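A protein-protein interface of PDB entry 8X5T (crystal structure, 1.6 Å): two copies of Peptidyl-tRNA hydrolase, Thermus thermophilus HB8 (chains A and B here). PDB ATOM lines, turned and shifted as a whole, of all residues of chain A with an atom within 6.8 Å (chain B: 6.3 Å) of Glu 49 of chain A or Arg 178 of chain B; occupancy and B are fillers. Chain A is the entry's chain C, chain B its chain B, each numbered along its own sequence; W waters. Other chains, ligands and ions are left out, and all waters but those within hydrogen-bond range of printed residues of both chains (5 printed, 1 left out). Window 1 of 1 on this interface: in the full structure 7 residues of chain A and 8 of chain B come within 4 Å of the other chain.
Water W5 lies within hydrogen-bond range of OE1 of Glu 49 of chain A and OE2 of Glu 162 of chain B.
Water W3 lies within hydrogen-bond range of the backbone carbonyl oxygen (O) of Leu 33 of chain A (2.7 Å), the backbone carbonyl oxygen (O) of Pro 174 of chain B (2.7 Å) and the guanidinium group (NH1) of Arg 178 of chain B (2.9 Å).
Water W4 lies within hydrogen-bond range of O of Glu 162 of chain B (2.7 Å), OE1 of Glu 49 of chain A (2.8 Å) and NH1 of Arg 169 of chain B (2.9 Å).
Water W2 lies within hydrogen-bond range of the indole nitrogen of Trp 165 of chain A (2.8 Å), the backbone carbonyl oxygen of Leu 33 of chain A (2.8 Å) and the backbone carbonyl oxygen of Gly 177 of chain B (3.1 Å).
Water W1 bridges OE1 of Glu 162 of chain B (2.8 Å) and O of Arg 169 of chain A (3.2 Å).
Positions printed for both chains: 165 and 169.
Of the 10 pairs that touch across the chains among the printed residues, none has its exchanged pair printed and touching as well.
The side-chain sulfur (SG) of Cys 166 of chain B is disulfide-bonded to the side-chain sulfur (SG) of Cys 175 of chain B (2.1 Å).
SG of Cys 166 of chain B sits at hydrogen-bond distance from NH2 of Arg 178 of chain B (3.3 Å).
The side-chain carboxylate (OE1) of Glu 170 of chain B lies within salt-bridge range of the guanidinium group (NH1) of Arg 178 of chain B, at 2.8 Å.
The side-chain carboxylate of Glu 162 of chain B lies within salt-bridge range of the guanidinium group of Arg 169 of chain A, at 2.6 Å.
NH2 of Arg 178 of chain B lies within salt-bridge range of OE2 of Glu 49 of chain A (2.9 Å).
The side-chain carboxylate (OE2) of Glu 49 of chain A sits close to the side-chain sulfur (SG) of Cys 166 of chain B (3.4 Å).
Pro 174 of chain B touches Gly 34 of chain A (CB to O, 3.7 Å).
NH1 of Arg 178 of chain B touches CD2 of Leu 35 of chain A, at 3.3 Å.
Glu 47 of chain A touches Glu 170 of chain B (O to OE2, 3.99 Å).
CA of Ala 48 of chain A touches OE2 of Glu 170 of chain B, 3.7 Å away.
CB of Ala 48 of chain A touches NH2 of Arg 178 of chain B, 3.6 Å away.
CE2 of Phe 179 of chain B touches OE2 of Glu 49 of chain A, at 3.7 Å.
Arg 178 of chain B touches Trp 165 of chain A (NE to CZ2, 3.5 Å).
Printed residues of chain B within 4 Å of Glu 49 of chain A: Cys 166 (3.4 Å), Arg 178 (2.9 Å) and Phe 179 (3.7 Å).
Printed residues of chain A within 4 Å of Cys 166 of chain B: Glu 49 (3.4 Å).
Of the printed residues of chain A, Glu 162 of chain B touches Arg 169.
Of the printed residues of chain B, Ala 48 of chain A touches Glu 170 and Arg 178.
Printed residues of chain B within 4 Å of Glu 47 of chain A: Glu 170 (3.99 Å).
Cys 175 of chain B touches none of the printed residues of chain A.
The nearest residue of chain A that does not touch Arg 178 of chain B is Gly 34 of chain A (4.6 Å).
The nearest printed residue of chain A that does not touch Glu 162 of chain B is Glu 49 of chain A (4.2 Å).
Of the 16 printed residues of chain B, 6 touch a printed residue of chain A.
Printed residues of chain B that touch a printed residue of chain A: Glu 162, Cys 166, Glu 170, Pro 174, Arg 178 and Phe 179.
Of the 16 printed residues of chain A, 7 touch a printed residue of chain B.
Hydrophobic or aromatic side chains of chain A that line the printed part of chain B: Leu 35, Ala 48 and Trp 165.
Along chain A the printed residues that touch a printed residue of chain B span positions 34 to 169.
Among the printed residues, 10 pairs touch across the chains.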
ATOM      1  N   MET A   5     -15.052  14.381  31.742  1.00  0.00           N
ATOM      2  CA  MET A   5     -14.450  13.279  31.068  1.00  0.00           C
ATOM      3  C   MET A   5     -13.061  13.614  30.588  1.00  0.00           C
ATOM      4  O   MET A   5     -12.254  12.712  30.249  1.00  0.00           O
ATOM      5  CB  MET A   5     -15.258  12.800  29.880  1.00  0.00           C
ATOM      6  CG  MET A   5     -16.583  12.112  30.298  1.00  0.00           C
ATOM      7  SD  MET A   5     -16.639  11.244  31.946  1.00  0.00           S
ATOM      8  CE  MET A   5     -15.902   9.651  31.415  1.00  0.00           C
ATOM      9  N   PHE A   6     -12.749  14.907  30.402  1.00  0.00           N
ATOM     10  CA  PHE A   6     -11.477  15.299  29.823  1.00  0.00           C
ATOM     11  C   PHE A   6     -11.086  16.704  30.262  1.00  0.00           C
ATOM     12  O   PHE A   6     -11.976  17.456  30.698  1.00  0.00           O
ATOM     13  CB  PHE A   6     -11.453  15.192  28.295  1.00  0.00           C
ATOM     14  CG  PHE A   6     -12.370  16.180  27.604  1.00  0.00           C
ATOM     15  CD1 PHE A   6     -12.019  17.484  27.413  1.00  0.00           C
ATOM     16  CD2 PHE A   6     -13.684  15.804  27.178  1.00  0.00           C
ATOM     17  CE1 PHE A   6     -12.854  18.401  26.830  1.00  0.00           C
ATOM     18  CE2 PHE A   6     -14.527  16.724  26.612  1.00  0.00           C
ATOM     19  CZ  PHE A   6     -14.147  18.001  26.439  1.00  0.00           C
ATOM     20  N   LEU A  33     -12.504  28.404  19.975  1.00  0.00           N
ATOM     21  CA  LEU A  33     -13.325  27.238  20.025  1.00  0.00           C
ATOM     22  C   LEU A  33     -14.812  27.587  20.165  1.00  0.00           C
ATOM     23  O   LEU A  33     -15.584  26.635  20.042  1.00  0.00           O
ATOM     24  CB  LEU A  33     -12.939  26.356  21.192  1.00  0.00           C
ATOM     25  CG  LEU A  33     -11.523  25.772  21.168  1.00  0.00           C
ATOM     26  CD1 LEU A  33     -11.204  25.014  22.466  1.00  0.00           C
ATOM     27  CD2 LEU A  33     -11.354  24.802  19.981  1.00  0.00           C
ATOM     28  N   GLY A  34     -15.158  28.806  20.394  1.00  0.00           N
ATOM     29  CA  GLY A  34     -16.610  29.204  20.518  1.00  0.00           C
ATOM     30  C   GLY A  34     -17.234  28.966  21.850  1.00  0.00           C
ATOM     31  O   GLY A  34     -18.422  28.887  21.980  1.00  0.00           O
ATOM     32  N   LEU A  35     -16.354  28.852  22.884  1.00  0.00           N
ATOM     33  CA  LEU A  35     -16.792  28.578  24.256  1.00  0.00           C
ATOM     34  C   LEU A  35     -17.062  29.774  25.110  1.00  0.00           C
ATOM     35  O   LEU A  35     -16.691  30.879  24.717  1.00  0.00           O
ATOM     36  CB  LEU A  35     -15.732  27.673  24.919  1.00  0.00           C
ATOM     37  CG  LEU A  35     -15.436  26.413  24.130  1.00  0.00           C
ATOM     38  CD1 LEU A  35     -14.464  25.531  24.858  1.00  0.00           C
ATOM     39  CD2 LEU A  35     -16.687  25.623  23.775  1.00  0.00           C
ATOM     40  N   SER A  36     -17.591  29.537  26.306  1.00  0.00           N
ATOM     41  CA  SER A  36     -17.860  30.622  27.228  1.00  0.00           C
ATOM     42  C   SER A  36     -16.986  30.419  28.512  1.00  0.00           C
ATOM     43  O   SER A  36     -17.328  29.601  29.378  1.00  0.00           O
ATOM     44  CB  SER A  36     -19.296  30.522  27.593  1.00  0.00           C
ATOM     45  OG  SER A  36     -19.671  31.578  28.527  1.00  0.00           O
ATOM     46  N   GLU A  47     -16.948  24.923  30.029  1.00  0.00           N
ATOM     47  CA  GLU A  47     -17.430  23.575  29.931  1.00  0.00           C
ATOM     48  C   GLU A  47     -18.025  23.323  28.535  1.00  0.00           C
ATOM     49  O   GLU A  47     -18.772  24.166  27.964  1.00  0.00           O
ATOM     50  CB  GLU A  47     -18.586  23.358  30.870  1.00  0.00           C
ATOM     51  CG  GLU A  47     -18.272  23.630  32.246  1.00  0.00           C
ATOM     52  CD  GLU A  47     -19.283  23.146  33.321  1.00  0.00           C
ATOM     53  OE1 GLU A  47     -19.910  22.052  33.139  1.00  0.00           O
ATOM     54  OE2 GLU A  47     -19.226  23.835  34.380  1.00  0.00           O
ATOM     55  N   ALA A  48     -17.726  22.159  27.996  1.00  0.00           N
ATOM     56  CA  ALA A  48     -18.285  21.764  26.699  1.00  0.00           C
ATOM     57  C   ALA A  48     -18.060  20.312  26.547  1.00  0.00           C
ATOM     58  O   ALA A  48     -17.025  19.706  26.857  1.00  0.00           O
ATOM     59  CB  ALA A  48     -17.658  22.449  25.583  1.00  0.00           C
ATOM     60  N   GLU A  49     -19.045  19.649  25.902  1.00  0.00           N
ATOM     61  CA  GLU A  49     -18.927  18.225  25.533  1.00  0.00           C
ATOM     62  C   GLU A  49     -18.552  17.257  26.656  1.00  0.00           C
ATOM     63  O   GLU A  49     -17.901  16.230  26.402  1.00  0.00           O
ATOM     64  CB  GLU A  49     -18.076  18.041  24.273  1.00  0.00           C
ATOM     65  CG  GLU A  49     -18.522  18.808  23.079  1.00  0.00           C
ATOM     66  CD  GLU A  49     -19.967  18.509  22.688  1.00  0.00           C
ATOM     67  OE1 GLU A  49     -20.195  17.301  22.573  1.00  0.00           O
ATOM     68  OE2 GLU A  49     -20.710  19.451  22.507  1.00  0.00           O
ATOM     69  N   GLY A  50     -18.929  17.605  27.869  1.00  0.00           N
ATOM     70  CA  GLY A  50     -18.685  16.786  29.002  1.00  0.00           C
ATOM     71  C   GLY A  50     -17.300  16.888  29.627  1.00  0.00           C
ATOM     72  O   GLY A  50     -16.915  16.076  30.483  1.00  0.00           O
ATOM     73  N   GLY A  51     -16.552  17.911  29.228  1.00  0.00           N
ATOM     74  CA  GLY A  51     -15.244  18.162  29.810  1.00  0.00           C
ATOM     75  C   GLY A  51     -15.016  19.641  29.987  1.00  0.00           C
ATOM     76  O   GLY A  51     -15.886  20.480  29.894  1.00  0.00           O
ATOM     77  N   LEU A  52     -13.792  19.928  30.417  1.00  0.00           N
ATOM     78  CA  LEU A  52     -13.367  21.307  30.780  1.00  0.00           C
ATOM     79  C   LEU A  52     -12.232  21.819  29.969  1.00  0.00           C
ATOM     80  O   LEU A  52     -11.317  21.026  29.624  1.00  0.00           O
ATOM     81  CB  LEU A  52     -12.940  21.385  32.269  1.00  0.00           C
ATOM     82  CG  LEU A  52     -14.070  21.074  33.267  1.00  0.00           C
ATOM     83  CD1 LEU A  52     -13.565  21.141  34.690  1.00  0.00           C
ATOM     84  CD2 LEU A  52     -15.267  21.967  33.172  1.00  0.00           C
ATOM     85  N   PHE A  53     -12.246  23.093  29.691  1.00  0.00           N
ATOM     86  CA  PHE A  53     -11.227  23.826  28.926  1.00  0.00           C
ATOM     87  C   PHE A  53     -10.698  24.894  29.825  1.00  0.00           C
ATOM     88  O   PHE A  53     -11.470  25.683  30.407  1.00  0.00           O
ATOM     89  CB  PHE A  53     -11.839  24.470  27.689  1.00  0.00           C
ATOM     90  CG  PHE A  53     -12.415  23.423  26.695  1.00  0.00           C
ATOM     91  CD1 PHE A  53     -13.576  22.771  26.945  1.00  0.00           C
ATOM     92  CD2 PHE A  53     -11.681  23.119  25.521  1.00  0.00           C
ATOM     93  CE1 PHE A  53     -14.038  21.743  26.058  1.00  0.00           C
ATOM     94  CE2 PHE A  53     -12.151  22.107  24.674  1.00  0.00           C
ATOM     95  CZ  PHE A  53     -13.308  21.481  24.955  1.00  0.00           C
ATOM     96  N   TRP A 165     -11.195  19.700  18.636  1.00  0.00           N
ATOM     97  CA  TRP A 165     -12.461  18.976  18.637  1.00  0.00           C
ATOM     98  C   TRP A 165     -12.395  17.556  18.195  1.00  0.00           C
ATOM     99  O   TRP A 165     -13.031  16.654  18.702  1.00  0.00           O
ATOM    100  CB  TRP A 165     -13.532  19.783  17.851  1.00  0.00           C
ATOM    101  CG  TRP A 165     -14.005  21.064  18.523  1.00  0.00           C
ATOM    102  CD1 TRP A 165     -13.941  22.317  18.031  1.00  0.00           C
ATOM    103  CD2 TRP A 165     -14.554  21.175  19.814  1.00  0.00           C
ATOM    104  NE1 TRP A 165     -14.466  23.198  18.869  1.00  0.00           N
ATOM    105  CE2 TRP A 165     -14.846  22.530  20.006  1.00  0.00           C
ATOM    106  CE3 TRP A 165     -14.927  20.255  20.809  1.00  0.00           C
ATOM    107  CZ2 TRP A 165     -15.454  23.003  21.200  1.00  0.00           C
ATOM    108  CZ3 TRP A 165     -15.480  20.746  22.018  1.00  0.00           C
ATOM    109  CH2 TRP A 165     -15.691  22.094  22.193  1.00  0.00           C
ATOM    110  N   VAL A 168     -11.171  15.593  21.172  1.00  0.00           N
ATOM    111  CA  VAL A 168     -12.225  15.412  22.151  1.00  0.00           C
ATOM    112  C   VAL A 168     -13.115  14.231  21.730  1.00  0.00           C
ATOM    113  O   VAL A 168     -13.498  13.454  22.553  1.00  0.00           O
ATOM    114  CB  VAL A 168     -13.068  16.706  22.242  1.00  0.00           C
ATOM    115  CG1 VAL A 168     -14.412  16.465  22.959  1.00  0.00           C
ATOM    116  CG2 VAL A 168     -12.287  17.819  22.974  1.00  0.00           C
ATOM    117  N   ARG A 169     -13.452  14.208  20.427  1.00  0.00           N
ATOM    118  CA  ARG A 169     -14.354  13.170  19.936  1.00  0.00           C
ATOM    119  C   ARG A 169     -13.722  11.828  19.652  1.00  0.00           C
ATOM    120  O   ARG A 169     -14.353  10.832  19.933  1.00  0.00           O
ATOM    121  CB  ARG A 169     -15.051  13.640  18.629  1.00  0.00           C
ATOM    122  CG  ARG A 169     -16.031  14.758  18.798  1.00  0.00           C
ATOM    123  CD  ARG A 169     -17.056  14.925  17.623  1.00  0.00           C
ATOM    124  NE  ARG A 169     -17.992  13.790  17.693  1.00  0.00           N
ATOM    125  CZ  ARG A 169     -18.006  12.747  16.827  1.00  0.00           C
ATOM    126  NH1 ARG A 169     -18.887  11.805  17.065  1.00  0.00           N
ATOM    127  NH2 ARG A 169     -17.211  12.673  15.788  1.00  0.00           N
ATOM    128  N   GLU B 162     -24.709  13.519  20.307  1.00  0.00           N
ATOM    129  CA  GLU B 162     -23.826  14.530  20.974  1.00  0.00           C
ATOM    130  C   GLU B 162     -24.326  15.940  20.700  1.00  0.00           C
ATOM    131  O   GLU B 162     -24.452  16.769  21.640  1.00  0.00           O
ATOM    132  CB  GLU B 162     -22.419  14.447  20.523  1.00  0.00           C
ATOM    133  CG  GLU B 162     -21.729  13.060  20.766  1.00  0.00           C
ATOM    134  CD  GLU B 162     -20.417  12.952  20.020  1.00  0.00           C
ATOM    135  OE1 GLU B 162     -20.020  11.741  19.838  1.00  0.00           O
ATOM    136  OE2 GLU B 162     -19.779  13.912  19.580  1.00  0.00           O
ATOM    137  N   ALA B 163     -24.687  16.165  19.450  1.00  0.00           N
ATOM    138  CA  ALA B 163     -25.193  17.470  19.058  1.00  0.00           C
ATOM    139  C   ALA B 163     -26.432  17.883  19.745  1.00  0.00           C
ATOM    140  O   ALA B 163     -26.639  19.057  20.130  1.00  0.00           O
ATOM    141  CB  ALA B 163     -25.281  17.535  17.539  1.00  0.00           C
ATOM    142  N   TRP B 165     -27.511  16.979  22.726  1.00  0.00           N
ATOM    143  CA  TRP B 165     -27.217  17.387  24.086  1.00  0.00           C
ATOM    144  C   TRP B 165     -26.424  18.685  24.153  1.00  0.00           C
ATOM    145  O   TRP B 165     -26.721  19.484  25.071  1.00  0.00           O
ATOM    146  CB  TRP B 165     -26.497  16.246  24.798  1.00  0.00           C
ATOM    147  CG  TRP B 165     -27.351  15.037  25.064  1.00  0.00           C
ATOM    148  CD1 TRP B 165     -27.066  13.823  24.627  1.00  0.00           C
ATOM    149  CD2 TRP B 165     -28.560  14.950  25.750  1.00  0.00           C
ATOM    150  NE1 TRP B 165     -28.037  12.950  25.028  1.00  0.00           N
ATOM    151  CE2 TRP B 165     -28.936  13.594  25.737  1.00  0.00           C
ATOM    152  CE3 TRP B 165     -29.310  15.819  26.452  1.00  0.00           C
ATOM    153  CZ2 TRP B 165     -30.092  13.153  26.337  1.00  0.00           C
ATOM    154  CZ3 TRP B 165     -30.522  15.359  27.130  1.00  0.00           C
ATOM    155  CH2 TRP B 165     -30.867  14.024  27.021  1.00  0.00           C
ATOM    156  N   CYS B 166     -25.593  18.910  23.187  1.00  0.00           N
ATOM    157  CA  CYS B 166     -24.897  20.203  23.095  1.00  0.00           C
ATOM    158  C   CYS B 166     -25.870  21.331  23.063  1.00  0.00           C
ATOM    159  O   CYS B 166     -25.863  22.338  23.759  1.00  0.00           O
ATOM    160  CB  CYS B 166     -23.958  20.213  21.943  1.00  0.00           C
ATOM    161  SG  CYS B 166     -23.011  21.781  21.768  1.00  0.00           S
ATOM    162  N   ARG B 169     -27.832  22.102  26.197  1.00  0.00           N
ATOM    163  CA  ARG B 169     -27.023  22.788  27.236  1.00  0.00           C
ATOM    164  C   ARG B 169     -26.578  24.166  26.834  1.00  0.00           C
ATOM    165  O   ARG B 169     -26.538  25.079  27.730  1.00  0.00           O
ATOM    166  CB  ARG B 169     -25.851  21.960  27.551  1.00  0.00           C
ATOM    167  CG  ARG B 169     -26.147  20.669  28.191  1.00  0.00           C
ATOM    168  CD  ARG B 169     -24.799  20.100  28.774  1.00  0.00           C
ATOM    169  NE  ARG B 169     -23.936  19.631  27.701  1.00  0.00           N
ATOM    170  CZ  ARG B 169     -23.913  18.395  27.141  1.00  0.00           C
ATOM    171  NH1 ARG B 169     -23.020  18.156  26.134  1.00  0.00           N
ATOM    172  NH2 ARG B 169     -24.655  17.338  27.642  1.00  0.00           N
ATOM    173  N   GLU B 170     -26.238  24.398  25.574  1.00  0.00           N
ATOM    174  CA  GLU B 170     -25.479  25.554  25.135  1.00  0.00           C
ATOM    175  C   GLU B 170     -26.163  26.441  24.124  1.00  0.00           C
ATOM    176  O   GLU B 170     -25.722  27.555  23.859  1.00  0.00           O
ATOM    177  CB  GLU B 170     -24.143  25.134  24.603  1.00  0.00           C
ATOM    178  CG  GLU B 170     -23.244  24.384  25.545  1.00  0.00           C
ATOM    179  CD  GLU B 170     -21.853  24.104  25.031  1.00  0.00           C
ATOM    180  OE1 GLU B 170     -21.217  24.955  24.371  1.00  0.00           O
ATOM    181  OE2 GLU B 170     -21.416  22.974  25.231  1.00  0.00           O
ATOM    182  N   PRO B 173     -25.434  28.582  18.546  1.00  0.00           N
ATOM    183  CA  PRO B 173     -24.134  28.992  17.983  1.00  0.00           C
ATOM    184  C   PRO B 173     -22.875  28.256  18.421  1.00  0.00           C
ATOM    185  O   PRO B 173     -22.050  27.919  17.567  1.00  0.00           O
ATOM    186  CB  PRO B 173     -24.142  30.507  18.283  1.00  0.00           C
ATOM    187  CG  PRO B 173     -25.596  30.893  18.315  1.00  0.00           C
ATOM    188  CD  PRO B 173     -26.254  29.698  19.000  1.00  0.00           C
ATOM    189  N   PRO B 174     -22.725  27.949  19.707  1.00  0.00           N
ATOM    190  CA  PRO B 174     -21.535  27.146  20.108  1.00  0.00           C
ATOM    191  C   PRO B 174     -21.470  25.765  19.458  1.00  0.00           C
ATOM    192  O   PRO B 174     -20.473  25.322  18.987  1.00  0.00           O
ATOM    193  CB  PRO B 174     -21.643  27.098  21.621  1.00  0.00           C
ATOM    194  CG  PRO B 174     -22.609  28.146  22.011  1.00  0.00           C
ATOM    195  CD  PRO B 174     -23.579  28.274  20.852  1.00  0.00           C
ATOM    196  N   CYS B 175     -22.663  25.134  19.449  1.00  0.00           N
ATOM    197  CA  CYS B 175     -22.774  23.803  18.899  1.00  0.00           C
ATOM    198  C   CYS B 175     -22.498  23.816  17.390  1.00  0.00           C
ATOM    199  O   CYS B 175     -21.800  22.931  16.862  1.00  0.00           O
ATOM    200  CB  CYS B 175     -24.113  23.213  19.303  1.00  0.00           C
ATOM    201  SG  CYS B 175     -24.367  23.156  21.079  1.00  0.00           S
ATOM    202  N   ALA B 176     -23.025  24.786  16.651  1.00  0.00           N
ATOM    203  CA  ALA B 176     -22.763  24.921  15.243  1.00  0.00           C
ATOM    204  C   ALA B 176     -21.237  25.018  14.967  1.00  0.00           C
ATOM    205  O   ALA B 176     -20.699  24.511  14.067  1.00  0.00           O
ATOM    206  CB  ALA B 176     -23.481  26.133  14.713  1.00  0.00           C
ATOM    207  N   GLY B 177     -20.590  25.774  15.884  1.00  0.00           N
ATOM    208  CA  GLY B 177     -19.133  26.036  15.748  1.00  0.00           C
ATOM    209  C   GLY B 177     -18.340  24.740  15.829  1.00  0.00           C
ATOM    210  O   GLY B 177     -17.256  24.749  15.296  1.00  0.00           O
ATOM    211  N   ARG B 178     -18.780  23.691  16.502  1.00  0.00           N
ATOM    212  CA  ARG B 178     -17.975  22.468  16.612  1.00  0.00           C
ATOM    213  C   ARG B 178     -18.505  21.312  15.816  1.00  0.00           C
ATOM    214  O   ARG B 178     -17.783  20.364  15.546  1.00  0.00           O
ATOM    215  CB  ARG B 178     -17.777  22.084  18.041  1.00  0.00           C
ATOM    216  CG  ARG B 178     -18.971  21.551  18.767  1.00  0.00           C
ATOM    217  CD  ARG B 178     -18.886  21.407  20.268  1.00  0.00           C
ATOM    218  NE  ARG B 178     -18.923  22.761  20.871  1.00  0.00           N
ATOM    219  CZ  ARG B 178     -19.386  23.072  22.049  1.00  0.00           C
ATOM    220  NH1 ARG B 178     -19.366  24.360  22.360  1.00  0.00           N
ATOM    221  NH2 ARG B 178     -19.957  22.207  22.832  1.00  0.00           N
ATOM    222  N   PHE B 179     -19.806  21.365  15.444  1.00  0.00           N
ATOM    223  CA  PHE B 179     -20.390  20.234  14.726  1.00  0.00           C
ATOM    224  C   PHE B 179     -20.535  20.517  13.232  1.00  0.00           C
ATOM    225  O   PHE B 179     -20.456  19.528  12.436  1.00  0.00           O
ATOM    226  CB  PHE B 179     -21.747  19.813  15.290  1.00  0.00           C
ATOM    227  CG  PHE B 179     -21.680  19.151  16.615  1.00  0.00           C
ATOM    228  CD1 PHE B 179     -21.338  17.769  16.697  1.00  0.00           C
ATOM    229  CD2 PHE B 179     -21.920  19.806  17.810  1.00  0.00           C
ATOM    230  CE1 PHE B 179     -21.256  17.142  17.890  1.00  0.00           C
ATOM    231  CE2 PHE B 179     -21.779  19.137  19.010  1.00  0.00           C
ATOM    232  CZ  PHE B 179     -21.456  17.808  19.045  1.00  0.00           C
ATOM    233  N   ASN B 180     -20.731  21.756  12.793  1.00  0.00           N
ATOM    234  CA  ASN B 180     -21.013  21.980  11.367  1.00  0.00           C
ATOM    235  C   ASN B 180     -19.932  21.589  10.444  1.00  0.00           C
ATOM    236  O   ASN B 180     -20.214  21.339   9.234  1.00  0.00           O
ATOM    237  CB  ASN B 180     -21.516  23.389  11.136  1.00  0.00           C
ATOM    238  CG  ASN B 180     -22.938  23.641  11.669  1.00  0.00           C
ATOM    239  OD1 ASN B 180     -23.501  22.931  12.475  1.00  0.00           O
ATOM    240  ND2 ASN B 180     -23.415  24.825  11.321  1.00  0.00           N
ATOM    241  N   GLY B 181     -18.694  21.604  10.906  1.00  0.00           N
ATOM    242  CA  GLY B 181     -17.678  21.285   9.950  1.00  0.00           C
ATOM    243  C   GLY B 181     -17.269  19.869   9.951  1.00  0.00           C
ATOM    244  O   GLY B 181     -16.320  19.587   9.227  1.00  0.00           O
ATOM    245  N   LEU B 182     -17.862  18.970  10.728  1.00  0.00           N
ATOM    246  CA  LEU B 182     -17.522  17.539  10.772  1.00  0.00           C
ATOM    247  C   LEU B 182     -17.827  16.867   9.414  1.00  0.00           C
ATOM    248  O   LEU B 182     -18.763  17.251   8.661  1.00  0.00           O
ATOM    249  CB  LEU B 182     -18.160  16.841  11.858  1.00  0.00           C
ATOM    250  CG  LEU B 182     -17.958  17.362  13.237  1.00  0.00           C
ATOM    251  CD1 LEU B 182     -18.603  16.442  14.186  1.00  0.00           C
ATOM    252  CD2 LEU B 182     -16.413  17.589  13.406  1.00  0.00           C
HETATM  253  O   HOH W   1     -17.372  11.596  20.755  1.00  0.00           O
HETATM  254  O   HOH W   2     -15.179  25.503  17.484  1.00  0.00           O
HETATM  255  O   HOH W   3     -17.984  25.461  20.012  1.00  0.00           O
HETATM  256  O   HOH W   4     -22.654  16.659  23.671  1.00  0.00           O
HETATM  257  O   HOH W   5     -18.582  15.793  21.187  1.00  0.00           O
